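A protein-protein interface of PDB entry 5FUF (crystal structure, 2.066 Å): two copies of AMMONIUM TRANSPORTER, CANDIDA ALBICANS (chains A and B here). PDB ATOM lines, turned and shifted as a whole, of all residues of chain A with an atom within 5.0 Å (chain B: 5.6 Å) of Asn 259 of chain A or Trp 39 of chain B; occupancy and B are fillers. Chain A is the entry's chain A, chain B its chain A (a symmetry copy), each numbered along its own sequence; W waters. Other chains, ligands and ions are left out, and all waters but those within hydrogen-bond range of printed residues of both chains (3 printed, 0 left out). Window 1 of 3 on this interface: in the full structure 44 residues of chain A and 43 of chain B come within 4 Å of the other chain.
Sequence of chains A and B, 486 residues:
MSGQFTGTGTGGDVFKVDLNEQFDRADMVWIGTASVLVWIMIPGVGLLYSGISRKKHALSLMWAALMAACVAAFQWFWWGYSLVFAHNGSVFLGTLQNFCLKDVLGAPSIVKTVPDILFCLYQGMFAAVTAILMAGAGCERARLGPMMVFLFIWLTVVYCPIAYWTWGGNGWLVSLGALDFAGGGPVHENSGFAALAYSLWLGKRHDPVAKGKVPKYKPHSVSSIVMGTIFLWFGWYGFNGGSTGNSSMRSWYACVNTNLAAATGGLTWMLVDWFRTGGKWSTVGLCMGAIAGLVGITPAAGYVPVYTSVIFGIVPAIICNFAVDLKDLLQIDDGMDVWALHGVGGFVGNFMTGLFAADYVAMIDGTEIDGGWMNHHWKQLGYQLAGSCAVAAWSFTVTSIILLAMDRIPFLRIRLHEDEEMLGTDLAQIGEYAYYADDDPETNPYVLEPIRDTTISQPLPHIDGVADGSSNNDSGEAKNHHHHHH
No position is printed for both chains.
Printed residues of chain B within 4 Å of Asn 259 of chain A: Trp 39 and Ala 73.
Of the printed residues of chain B, Ala 263 of chain A touches Ala 73.
Printed residues of chain B within 4 Å of Ile 230 of chain A: Trp 39 (3.7 Å) and Pro 43 (3.4 Å).
Of the printed residues of chain A, Val 36 of chain B touches Phe 234 (3.4 Å) and Tyr 237 (3.5 Å).
Val 38 of chain B touches none of the printed residues of chain A.
Asn 257 of chain A touches none of the printed residues of chain B.
The nearest printed residue of chain A that does not touch Leu 66 of chain B is Ile 230 of chain A (4.2 Å).
Hydrophobic or aromatic side chains of chain B within 4 Å of the printed part of chain A: Val 36, Trp 39, Ile 40, Pro 43, Leu 66, Ala 73, Leu 121 and Met 125.
Of the 14 printed residues of chain A, 10 touch a printed residue of chain B.
Printed residues of chain A that touch a printed residue of chain B: Thr 229, Ile 230, Trp 233, Phe 234, Tyr 237, Cys 255, Val 256, Asn 259, Leu 260 and Ala 263.
Hydrophobic or aromatic side chains of chain A that line the printed part of chain B: Ile 230, Trp 233, Phe 234, Tyr 237, Val 256, Leu 260 and Ala 263.
Along chain A the printed residues that touch a printed residue of chain B span positions 229 to 263.
Water W3 lies within hydrogen-bond range of the side-chain amide oxygen (OD1) of Asn 259 of chain A, the indole nitrogen (NE1) of Trp 39 of chain B and the backbone carbonyl oxygen (O) of Ala 69 of chain B.
Water W2 lies within hydrogen-bond range of the backbone carbonyl oxygen of Leu 121 of chain B (2.9 Å), the side-chain amide nitrogen of Asn 259 of chain A (3.3 Å) and the side-chain sulfur of Met 125 of chain B (3.6 Å).
Water W1 bridges ND2 of Asn 259 of chain A (2.9 Å) and SD of Met 125 of chain B (3.6 Å).
Among the printed residues, merely in contact across the chains: Trp 233 of chain A with Trp 39 of chain B, Tyr 237 of chain A with Trp 39 of chain B, Ile 230 of chain A with Pro 43 of chain B, Phe 234 of chain A with Val 36 of chain B, Tyr 237 of chain A with Val 36 of chain B, Tyr 237 of chain A with Met 125 of chain B, Ala 263 of chain A with Ala 73 of chain B, Asn 259 of chain A with Ala 73 of chain B, Ile 230 of chain A with Trp 39 of chain B, Cys 255 of chain A with Leu 121 of chain B, Val 256 of chain A with Leu 121 of chain B, Leu 260 of chain A with Ala 73 of chain B, Phe 234 of chain A with Ile 40 of chain B, Thr 229 of chain A with Leu 66 of chain B and Asn 259 of chain A with Trp 39 of chain B.
The indole nitrogen (NE1) of Trp 233 of chain A lies within hydrogen-bond range of the side-chain hydroxyl (OH) of Tyr 237 of chain A, at 3.2 Å.
NE1 of Trp 233 of chain A lies close to OD1 of Asn 259 of chain A, at 3.4 Å.
OH of Tyr 237 of chain A is in hydrogen-bond range of OD1 of Asn 259 of chain A, at 3.1 Å.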
ATOM      1  N   THR A 229      21.207 -19.035  30.235  1.00  0.00           N
ATOM      2  CA  THR A 229      19.807 -18.828  30.603  1.00  0.00           C
ATOM      3  C   THR A 229      18.906 -19.925  30.045  1.00  0.00           C
ATOM      4  O   THR A 229      17.941 -20.335  30.716  1.00  0.00           O
ATOM      5  CB  THR A 229      19.348 -17.449  30.123  1.00  0.00           C
ATOM      6  OG1 THR A 229      20.244 -16.452  30.631  1.00  0.00           O
ATOM      7  CG2 THR A 229      17.945 -17.128  30.627  1.00  0.00           C
ATOM      8  N   ILE A 230      19.199 -20.409  28.831  1.00  0.00           N
ATOM      9  CA  ILE A 230      18.455 -21.536  28.266  1.00  0.00           C
ATOM     10  C   ILE A 230      18.548 -22.754  29.187  1.00  0.00           C
ATOM     11  O   ILE A 230      17.524 -23.340  29.568  1.00  0.00           O
ATOM     12  CB  ILE A 230      18.959 -21.867  26.848  1.00  0.00           C
ATOM     13  CG1 ILE A 230      18.543 -20.779  25.847  1.00  0.00           C
ATOM     14  CG2 ILE A 230      18.479 -23.269  26.409  1.00  0.00           C
ATOM     15  CD1 ILE A 230      19.346 -20.828  24.528  1.00  0.00           C
ATOM     16  N   TRP A 233      16.618 -22.102  32.709  1.00  0.00           N
ATOM     17  CA  TRP A 233      15.172 -22.143  32.605  1.00  0.00           C
ATOM     18  C   TRP A 233      14.698 -23.578  32.341  1.00  0.00           C
ATOM     19  O   TRP A 233      13.798 -24.043  32.949  1.00  0.00           O
ATOM     20  CB  TRP A 233      14.736 -21.164  31.519  1.00  0.00           C
ATOM     21  CG  TRP A 233      13.299 -20.806  31.404  1.00  0.00           C
ATOM     22  CD1 TRP A 233      12.249 -21.558  31.731  1.00  0.00           C
ATOM     23  CD2 TRP A 233      12.770 -19.590  30.884  1.00  0.00           C
ATOM     24  NE1 TRP A 233      11.101 -20.902  31.468  1.00  0.00           N
ATOM     25  CE2 TRP A 233      11.395 -19.686  30.941  1.00  0.00           C
ATOM     26  CE3 TRP A 233      13.334 -18.426  30.382  1.00  0.00           C
ATOM     27  CZ2 TRP A 233      10.575 -18.678  30.510  1.00  0.00           C
ATOM     28  CZ3 TRP A 233      12.515 -17.435  29.957  1.00  0.00           C
ATOM     29  CH2 TRP A 233      11.158 -17.558  30.027  1.00  0.00           C
ATOM     30  N   PHE A 234      15.355 -24.261  31.431  1.00  0.00           N
ATOM     31  CA  PHE A 234      15.046 -25.633  31.093  1.00  0.00           C
ATOM     32  C   PHE A 234      15.144 -26.528  32.320  1.00  0.00           C
ATOM     33  O   PHE A 234      14.256 -27.261  32.600  1.00  0.00           O
ATOM     34  CB  PHE A 234      15.963 -26.082  29.959  1.00  0.00           C
ATOM     35  CG  PHE A 234      15.882 -27.531  29.597  1.00  0.00           C
ATOM     36  CD1 PHE A 234      14.838 -28.020  28.877  1.00  0.00           C
ATOM     37  CD2 PHE A 234      16.907 -28.380  29.904  1.00  0.00           C
ATOM     38  CE1 PHE A 234      14.792 -29.339  28.508  1.00  0.00           C
ATOM     39  CE2 PHE A 234      16.870 -29.697  29.549  1.00  0.00           C
ATOM     40  CZ  PHE A 234      15.805 -30.181  28.849  1.00  0.00           C
ATOM     41  N   TYR A 237      12.581 -26.422  35.608  1.00  0.00           N
ATOM     42  CA  TYR A 237      11.360 -27.190  35.677  1.00  0.00           C
ATOM     43  C   TYR A 237      11.573 -28.377  36.621  1.00  0.00           C
ATOM     44  O   TYR A 237      10.688 -28.743  37.324  1.00  0.00           O
ATOM     45  CB  TYR A 237      10.874 -27.605  34.304  1.00  0.00           C
ATOM     46  CG  TYR A 237      10.393 -26.462  33.455  1.00  0.00           C
ATOM     47  CD1 TYR A 237       9.242 -25.773  33.766  1.00  0.00           C
ATOM     48  CD2 TYR A 237      11.085 -26.086  32.339  1.00  0.00           C
ATOM     49  CE1 TYR A 237       8.808 -24.739  32.992  1.00  0.00           C
ATOM     50  CE2 TYR A 237      10.652 -25.061  31.552  1.00  0.00           C
ATOM     51  CZ  TYR A 237       9.512 -24.386  31.887  1.00  0.00           C
ATOM     52  OH  TYR A 237       9.106 -23.367  31.102  1.00  0.00           O
ATOM     53  N   CYS A 255       5.313 -25.825  37.892  1.00  0.00           N
ATOM     54  CA  CYS A 255       5.967 -25.539  36.613  1.00  0.00           C
ATOM     55  C   CYS A 255       5.317 -24.350  35.899  1.00  0.00           C
ATOM     56  O   CYS A 255       6.015 -23.539  35.280  1.00  0.00           O
ATOM     57  CB  CYS A 255       5.938 -26.785  35.723  1.00  0.00           C
ATOM     58  SG  CYS A 255       7.070 -28.121  36.267  1.00  0.00           S
ATOM     59  N   VAL A 256       3.981 -24.246  35.942  1.00  0.00           N
ATOM     60  CA  VAL A 256       3.309 -23.073  35.381  1.00  0.00           C
ATOM     61  C   VAL A 256       3.783 -21.806  36.089  1.00  0.00           C
ATOM     62  O   VAL A 256       4.136 -20.807  35.441  1.00  0.00           O
ATOM     63  CB  VAL A 256       1.773 -23.233  35.467  1.00  0.00           C
ATOM     64  CG1 VAL A 256       1.069 -21.925  35.039  1.00  0.00           C
ATOM     65  CG2 VAL A 256       1.308 -24.407  34.600  1.00  0.00           C
ATOM     66  N   ASN A 257       3.827 -21.833  37.429  1.00  0.00           N
ATOM     67  CA  ASN A 257       4.321 -20.681  38.177  1.00  0.00           C
ATOM     68  C   ASN A 257       5.760 -20.345  37.793  1.00  0.00           C
ATOM     69  O   ASN A 257       6.121 -19.169  37.684  1.00  0.00           O
ATOM     70  CB  ASN A 257       4.245 -20.933  39.680  1.00  0.00           C
ATOM     71  CG  ASN A 257       2.822 -20.776  40.247  1.00  0.00           C
ATOM     72  OD1 ASN A 257       1.943 -20.190  39.608  1.00  0.00           O
ATOM     73  ND2 ASN A 257       2.611 -21.285  41.460  1.00  0.00           N
ATOM     74  N   THR A 258       6.599 -21.371  37.633  1.00  0.00           N
ATOM     75  CA  THR A 258       8.004 -21.156  37.284  1.00  0.00           C
ATOM     76  C   THR A 258       8.134 -20.456  35.936  1.00  0.00           C
ATOM     77  O   THR A 258       8.868 -19.471  35.800  1.00  0.00           O
ATOM     78  CB  THR A 258       8.736 -22.504  37.270  1.00  0.00           C
ATOM     79  OG1 THR A 258       8.662 -23.099  38.576  1.00  0.00           O
ATOM     80  CG2 THR A 258      10.200 -22.335  36.882  1.00  0.00           C
ATOM     81  N   ASN A 259       7.436 -20.971  34.925  1.00  0.00           N
ATOM     82  CA  ASN A 259       7.477 -20.393  33.588  1.00  0.00           C
ATOM     83  C   ASN A 259       7.009 -18.937  33.608  1.00  0.00           C
ATOM     84  O   ASN A 259       7.649 -18.059  33.015  1.00  0.00           O
ATOM     85  CB  ASN A 259       6.605 -21.254  32.664  1.00  0.00           C
ATOM     86  CG  ASN A 259       6.721 -20.874  31.186  1.00  0.00           C
ATOM     87  OD1 ASN A 259       7.803 -20.533  30.682  1.00  0.00           O
ATOM     88  ND2 ASN A 259       5.589 -20.923  30.490  1.00  0.00           N
ATOM     89  N   LEU A 260       5.913 -18.660  34.324  1.00  0.00           N
ATOM     90  CA  LEU A 260       5.319 -17.325  34.299  1.00  0.00           C
ATOM     91  C   LEU A 260       6.186 -16.304  35.035  1.00  0.00           C
ATOM     92  O   LEU A 260       6.323 -15.158  34.585  1.00  0.00           O
ATOM     93  CB  LEU A 260       3.907 -17.388  34.887  1.00  0.00           C
ATOM     94  CG  LEU A 260       2.983 -16.186  34.688  1.00  0.00           C
ATOM     95  CD1 LEU A 260       2.923 -15.757  33.219  1.00  0.00           C
ATOM     96  CD2 LEU A 260       1.575 -16.523  35.216  1.00  0.00           C
ATOM     97  N   ALA A 261       6.798 -16.701  36.154  1.00  0.00           N
ATOM     98  CA  ALA A 261       7.670 -15.781  36.884  1.00  0.00           C
ATOM     99  C   ALA A 261       8.901 -15.417  36.065  1.00  0.00           C
ATOM    100  O   ALA A 261       9.369 -14.266  36.100  1.00  0.00           O
ATOM    101  CB  ALA A 261       8.086 -16.399  38.219  1.00  0.00           C
ATOM    102  N   ALA A 262       9.450 -16.392  35.334  1.00  0.00           N
ATOM    103  CA  ALA A 262      10.605 -16.133  34.470  1.00  0.00           C
ATOM    104  C   ALA A 262      10.241 -15.187  33.337  1.00  0.00           C
ATOM    105  O   ALA A 262      10.986 -14.242  33.027  1.00  0.00           O
ATOM    106  CB  ALA A 262      11.116 -17.453  33.894  1.00  0.00           C
ATOM    107  N   ALA A 263       9.114 -15.462  32.684  1.00  0.00           N
ATOM    108  CA  ALA A 263       8.615 -14.619  31.604  1.00  0.00           C
ATOM    109  C   ALA A 263       8.418 -13.179  32.070  1.00  0.00           C
ATOM    110  O   ALA A 263       8.925 -12.233  31.449  1.00  0.00           O
ATOM    111  CB  ALA A 263       7.296 -15.210  31.079  1.00  0.00           C
ATOM    112  N   ALA B  34       7.273 -34.120  28.709  1.00  0.00           N
ATOM    113  CA  ALA B  34       7.159 -33.673  27.332  1.00  0.00           C
ATOM    114  C   ALA B  34       7.064 -32.148  27.250  1.00  0.00           C
ATOM    115  O   ALA B  34       7.546 -31.556  26.277  1.00  0.00           O
ATOM    116  CB  ALA B  34       5.952 -34.348  26.653  1.00  0.00           C
ATOM    117  N   SER B  35       6.475 -31.497  28.275  1.00  0.00           N
ATOM    118  CA  SER B  35       6.382 -30.033  28.273  1.00  0.00           C
ATOM    119  C   SER B  35       7.759 -29.393  28.363  1.00  0.00           C
ATOM    120  O   SER B  35       8.022 -28.378  27.715  1.00  0.00           O
ATOM    121  CB  SER B  35       5.514 -29.523  29.434  1.00  0.00           C
ATOM    122  OG  SER B  35       4.225 -30.153  29.464  1.00  0.00           O
ATOM    123  N   VAL B  36       8.632 -29.957  29.203  1.00  0.00           N
ATOM    124  CA  VAL B  36       9.995 -29.453  29.333  1.00  0.00           C
ATOM    125  C   VAL B  36      10.748 -29.619  28.015  1.00  0.00           C
ATOM    126  O   VAL B  36      11.458 -28.704  27.565  1.00  0.00           O
ATOM    127  CB  VAL B  36      10.697 -30.165  30.510  1.00  0.00           C
ATOM    128  CG1 VAL B  36      12.132 -29.692  30.659  1.00  0.00           C
ATOM    129  CG2 VAL B  36       9.919 -29.898  31.808  1.00  0.00           C
ATOM    130  N   LEU B  37      10.567 -30.772  27.356  1.00  0.00           N
ATOM    131  CA  LEU B  37      11.200 -31.017  26.060  1.00  0.00           C
ATOM    132  C   LEU B  37      10.758 -30.002  25.004  1.00  0.00           C
ATOM    133  O   LEU B  37      11.590 -29.487  24.247  1.00  0.00           O
ATOM    134  CB  LEU B  37      10.892 -32.446  25.601  1.00  0.00           C
ATOM    135  CG  LEU B  37      11.546 -33.527  26.489  1.00  0.00           C
ATOM    136  CD1 LEU B  37      11.075 -34.928  26.154  1.00  0.00           C
ATOM    137  CD2 LEU B  37      13.078 -33.456  26.360  1.00  0.00           C
ATOM    138  N   VAL B  38       9.457 -29.702  24.928  1.00  0.00           N
ATOM    139  CA  VAL B  38       9.032 -28.714  23.941  1.00  0.00           C
ATOM    140  C   VAL B  38       9.646 -27.351  24.248  1.00  0.00           C
ATOM    141  O   VAL B  38       9.994 -26.606  23.318  1.00  0.00           O
ATOM    142  CB  VAL B  38       7.496 -28.626  23.835  1.00  0.00           C
ATOM    143  CG1 VAL B  38       7.088 -27.611  22.749  1.00  0.00           C
ATOM    144  CG2 VAL B  38       6.903 -29.994  23.474  1.00  0.00           C
ATOM    145  N   TRP B  39       9.807 -27.001  25.537  1.00  0.00           N
ATOM    146  CA  TRP B  39      10.318 -25.668  25.855  1.00  0.00           C
ATOM    147  C   TRP B  39      11.668 -25.427  25.179  1.00  0.00           C
ATOM    148  O   TRP B  39      11.900 -24.351  24.614  1.00  0.00           O
ATOM    149  CB  TRP B  39      10.416 -25.426  27.378  1.00  0.00           C
ATOM    150  CG  TRP B  39      10.725 -23.978  27.653  1.00  0.00           C
ATOM    151  CD1 TRP B  39       9.826 -22.956  27.832  1.00  0.00           C
ATOM    152  CD2 TRP B  39      12.033 -23.365  27.673  1.00  0.00           C
ATOM    153  NE1 TRP B  39      10.499 -21.749  27.989  1.00  0.00           N
ATOM    154  CE2 TRP B  39      11.849 -21.980  27.908  1.00  0.00           C
ATOM    155  CE3 TRP B  39      13.335 -23.862  27.562  1.00  0.00           C
ATOM    156  CZ2 TRP B  39      12.925 -21.085  28.008  1.00  0.00           C
ATOM    157  CZ3 TRP B  39      14.410 -22.974  27.666  1.00  0.00           C
ATOM    158  CH2 TRP B  39      14.195 -21.602  27.877  1.00  0.00           C
ATOM    159  N   ILE B  40      12.547 -26.438  25.154  1.00  0.00           N
ATOM    160  CA  ILE B  40      13.873 -26.213  24.577  1.00  0.00           C
ATOM    161  C   ILE B  40      13.849 -26.150  23.055  1.00  0.00           C
ATOM    162  O   ILE B  40      14.817 -25.670  22.445  1.00  0.00           O
ATOM    163  CB  ILE B  40      14.894 -27.263  25.081  1.00  0.00           C
ATOM    164  CG1 ILE B  40      16.330 -26.685  24.997  1.00  0.00           C
ATOM    165  CG2 ILE B  40      14.782 -28.565  24.297  1.00  0.00           C
ATOM    166  CD1 ILE B  40      17.395 -27.534  25.711  1.00  0.00           C
ATOM    167  N   MET B  41      12.739 -26.544  22.421  1.00  0.00           N
ATOM    168  CA  MET B  41      12.582 -26.260  20.995  1.00  0.00           C
ATOM    169  C   MET B  41      12.536 -24.766  20.702  1.00  0.00           C
ATOM    170  O   MET B  41      12.824 -24.371  19.572  1.00  0.00           O
ATOM    171  CB  MET B  41      11.312 -26.913  20.447  1.00  0.00           C
ATOM    172  CG  MET B  41      11.359 -28.440  20.482  1.00  0.00           C
ATOM    173  SD  MET B  41       9.783 -29.186  19.995  1.00  0.00           S
ATOM    174  CE  MET B  41       9.688 -28.696  18.270  1.00  0.00           C
ATOM    175  N   ILE B  42      12.154 -23.939  21.678  1.00  0.00           N
ATOM    176  CA  ILE B  42      12.049 -22.495  21.441  1.00  0.00           C
ATOM    177  C   ILE B  42      13.414 -21.911  21.056  1.00  0.00           C
ATOM    178  O   ILE B  42      13.514 -21.302  19.984  1.00  0.00           O
ATOM    179  CB  ILE B  42      11.389 -21.790  22.625  1.00  0.00           C
ATOM    180  CG1 ILE B  42       9.999 -22.382  22.917  1.00  0.00           C
ATOM    181  CG2 ILE B  42      11.281 -20.259  22.370  1.00  0.00           C
ATOM    182  CD1 ILE B  42       9.517 -22.128  24.358  1.00  0.00           C
ATOM    183  N   PRO B  43      14.485 -22.075  21.857  1.00  0.00           N
ATOM    184  CA  PRO B  43      15.807 -21.647  21.371  1.00  0.00           C
ATOM    185  C   PRO B  43      16.302 -22.476  20.218  1.00  0.00           C
ATOM    186  O   PRO B  43      17.131 -21.983  19.451  1.00  0.00           O
ATOM    187  CB  PRO B  43      16.714 -21.815  22.595  1.00  0.00           C
ATOM    188  CG  PRO B  43      15.987 -22.860  23.466  1.00  0.00           C
ATOM    189  CD  PRO B  43      14.549 -22.530  23.260  1.00  0.00           C
ATOM    190  N   LEU B  66      14.417 -16.227  23.652  1.00  0.00           N
ATOM    191  CA  LEU B  66      14.080 -15.966  25.050  1.00  0.00           C
ATOM    192  C   LEU B  66      13.033 -14.867  25.163  1.00  0.00           C
ATOM    193  O   LEU B  66      12.113 -14.958  25.988  1.00  0.00           O
ATOM    194  CB  LEU B  66      15.336 -15.596  25.838  1.00  0.00           C
ATOM    195  CG  LEU B  66      16.341 -16.736  26.020  1.00  0.00           C
ATOM    196  CD1 LEU B  66      17.548 -16.233  26.783  1.00  0.00           C
ATOM    197  CD2 LEU B  66      15.677 -17.873  26.770  1.00  0.00           C
ATOM    198  N   ALA B  69       9.782 -16.572  24.321  1.00  0.00           N
ATOM    199  CA  ALA B  69       9.335 -17.376  25.451  1.00  0.00           C
ATOM    200  C   ALA B  69       8.653 -16.518  26.510  1.00  0.00           C
ATOM    201  O   ALA B  69       7.646 -16.945  27.093  1.00  0.00           O
ATOM    202  CB  ALA B  69      10.514 -18.139  26.056  1.00  0.00           C
ATOM    203  N   ALA B  73       4.557 -16.790  27.027  1.00  0.00           N
ATOM    204  CA  ALA B  73       4.074 -17.276  28.318  1.00  0.00           C
ATOM    205  C   ALA B  73       3.095 -16.288  28.946  1.00  0.00           C
ATOM    206  O   ALA B  73       2.094 -16.694  29.559  1.00  0.00           O
ATOM    207  CB  ALA B  73       5.244 -17.549  29.258  1.00  0.00           C
ATOM    208  N   LEU B 121       0.216 -26.114  30.791  1.00  0.00           N
ATOM    209  CA  LEU B 121       1.675 -26.087  30.697  1.00  0.00           C
ATOM    210  C   LEU B 121       2.149 -26.636  29.355  1.00  0.00           C
ATOM    211  O   LEU B 121       3.003 -26.030  28.680  1.00  0.00           O
ATOM    212  CB  LEU B 121       2.282 -26.903  31.843  1.00  0.00           C
ATOM    213  CG  LEU B 121       3.818 -27.048  31.818  1.00  0.00           C
ATOM    214  CD1 LEU B 121       4.494 -25.744  32.254  1.00  0.00           C
ATOM    215  CD2 LEU B 121       4.250 -28.213  32.710  1.00  0.00           C
ATOM    216  N   MET B 125       3.608 -24.438  25.553  1.00  0.00           N
ATOM    217  CA  MET B 125       4.892 -24.555  24.868  1.00  0.00           C
ATOM    218  C   MET B 125       4.711 -24.540  23.355  1.00  0.00           C
ATOM    219  O   MET B 125       5.564 -24.016  22.637  1.00  0.00           O
ATOM    220  CB  MET B 125       5.612 -25.834  25.303  1.00  0.00           C
ATOM    221  CG  MET B 125       5.721 -26.000  26.814  1.00  0.00           C
ATOM    222  SD  MET B 125       6.589 -24.620  27.580  1.00  0.00           S
ATOM    223  CE  MET B 125       6.635 -25.229  29.272  1.00  0.00           C
HETATM  224  O   HOH W   1       5.789 -21.149  27.590  1.00  0.00           O
HETATM  225  O   HOH W   2       3.608 -23.221  29.078  1.00  0.00           O
HETATM  226  O   HOH W   3       8.187 -19.883  28.039  1.00  0.00           O
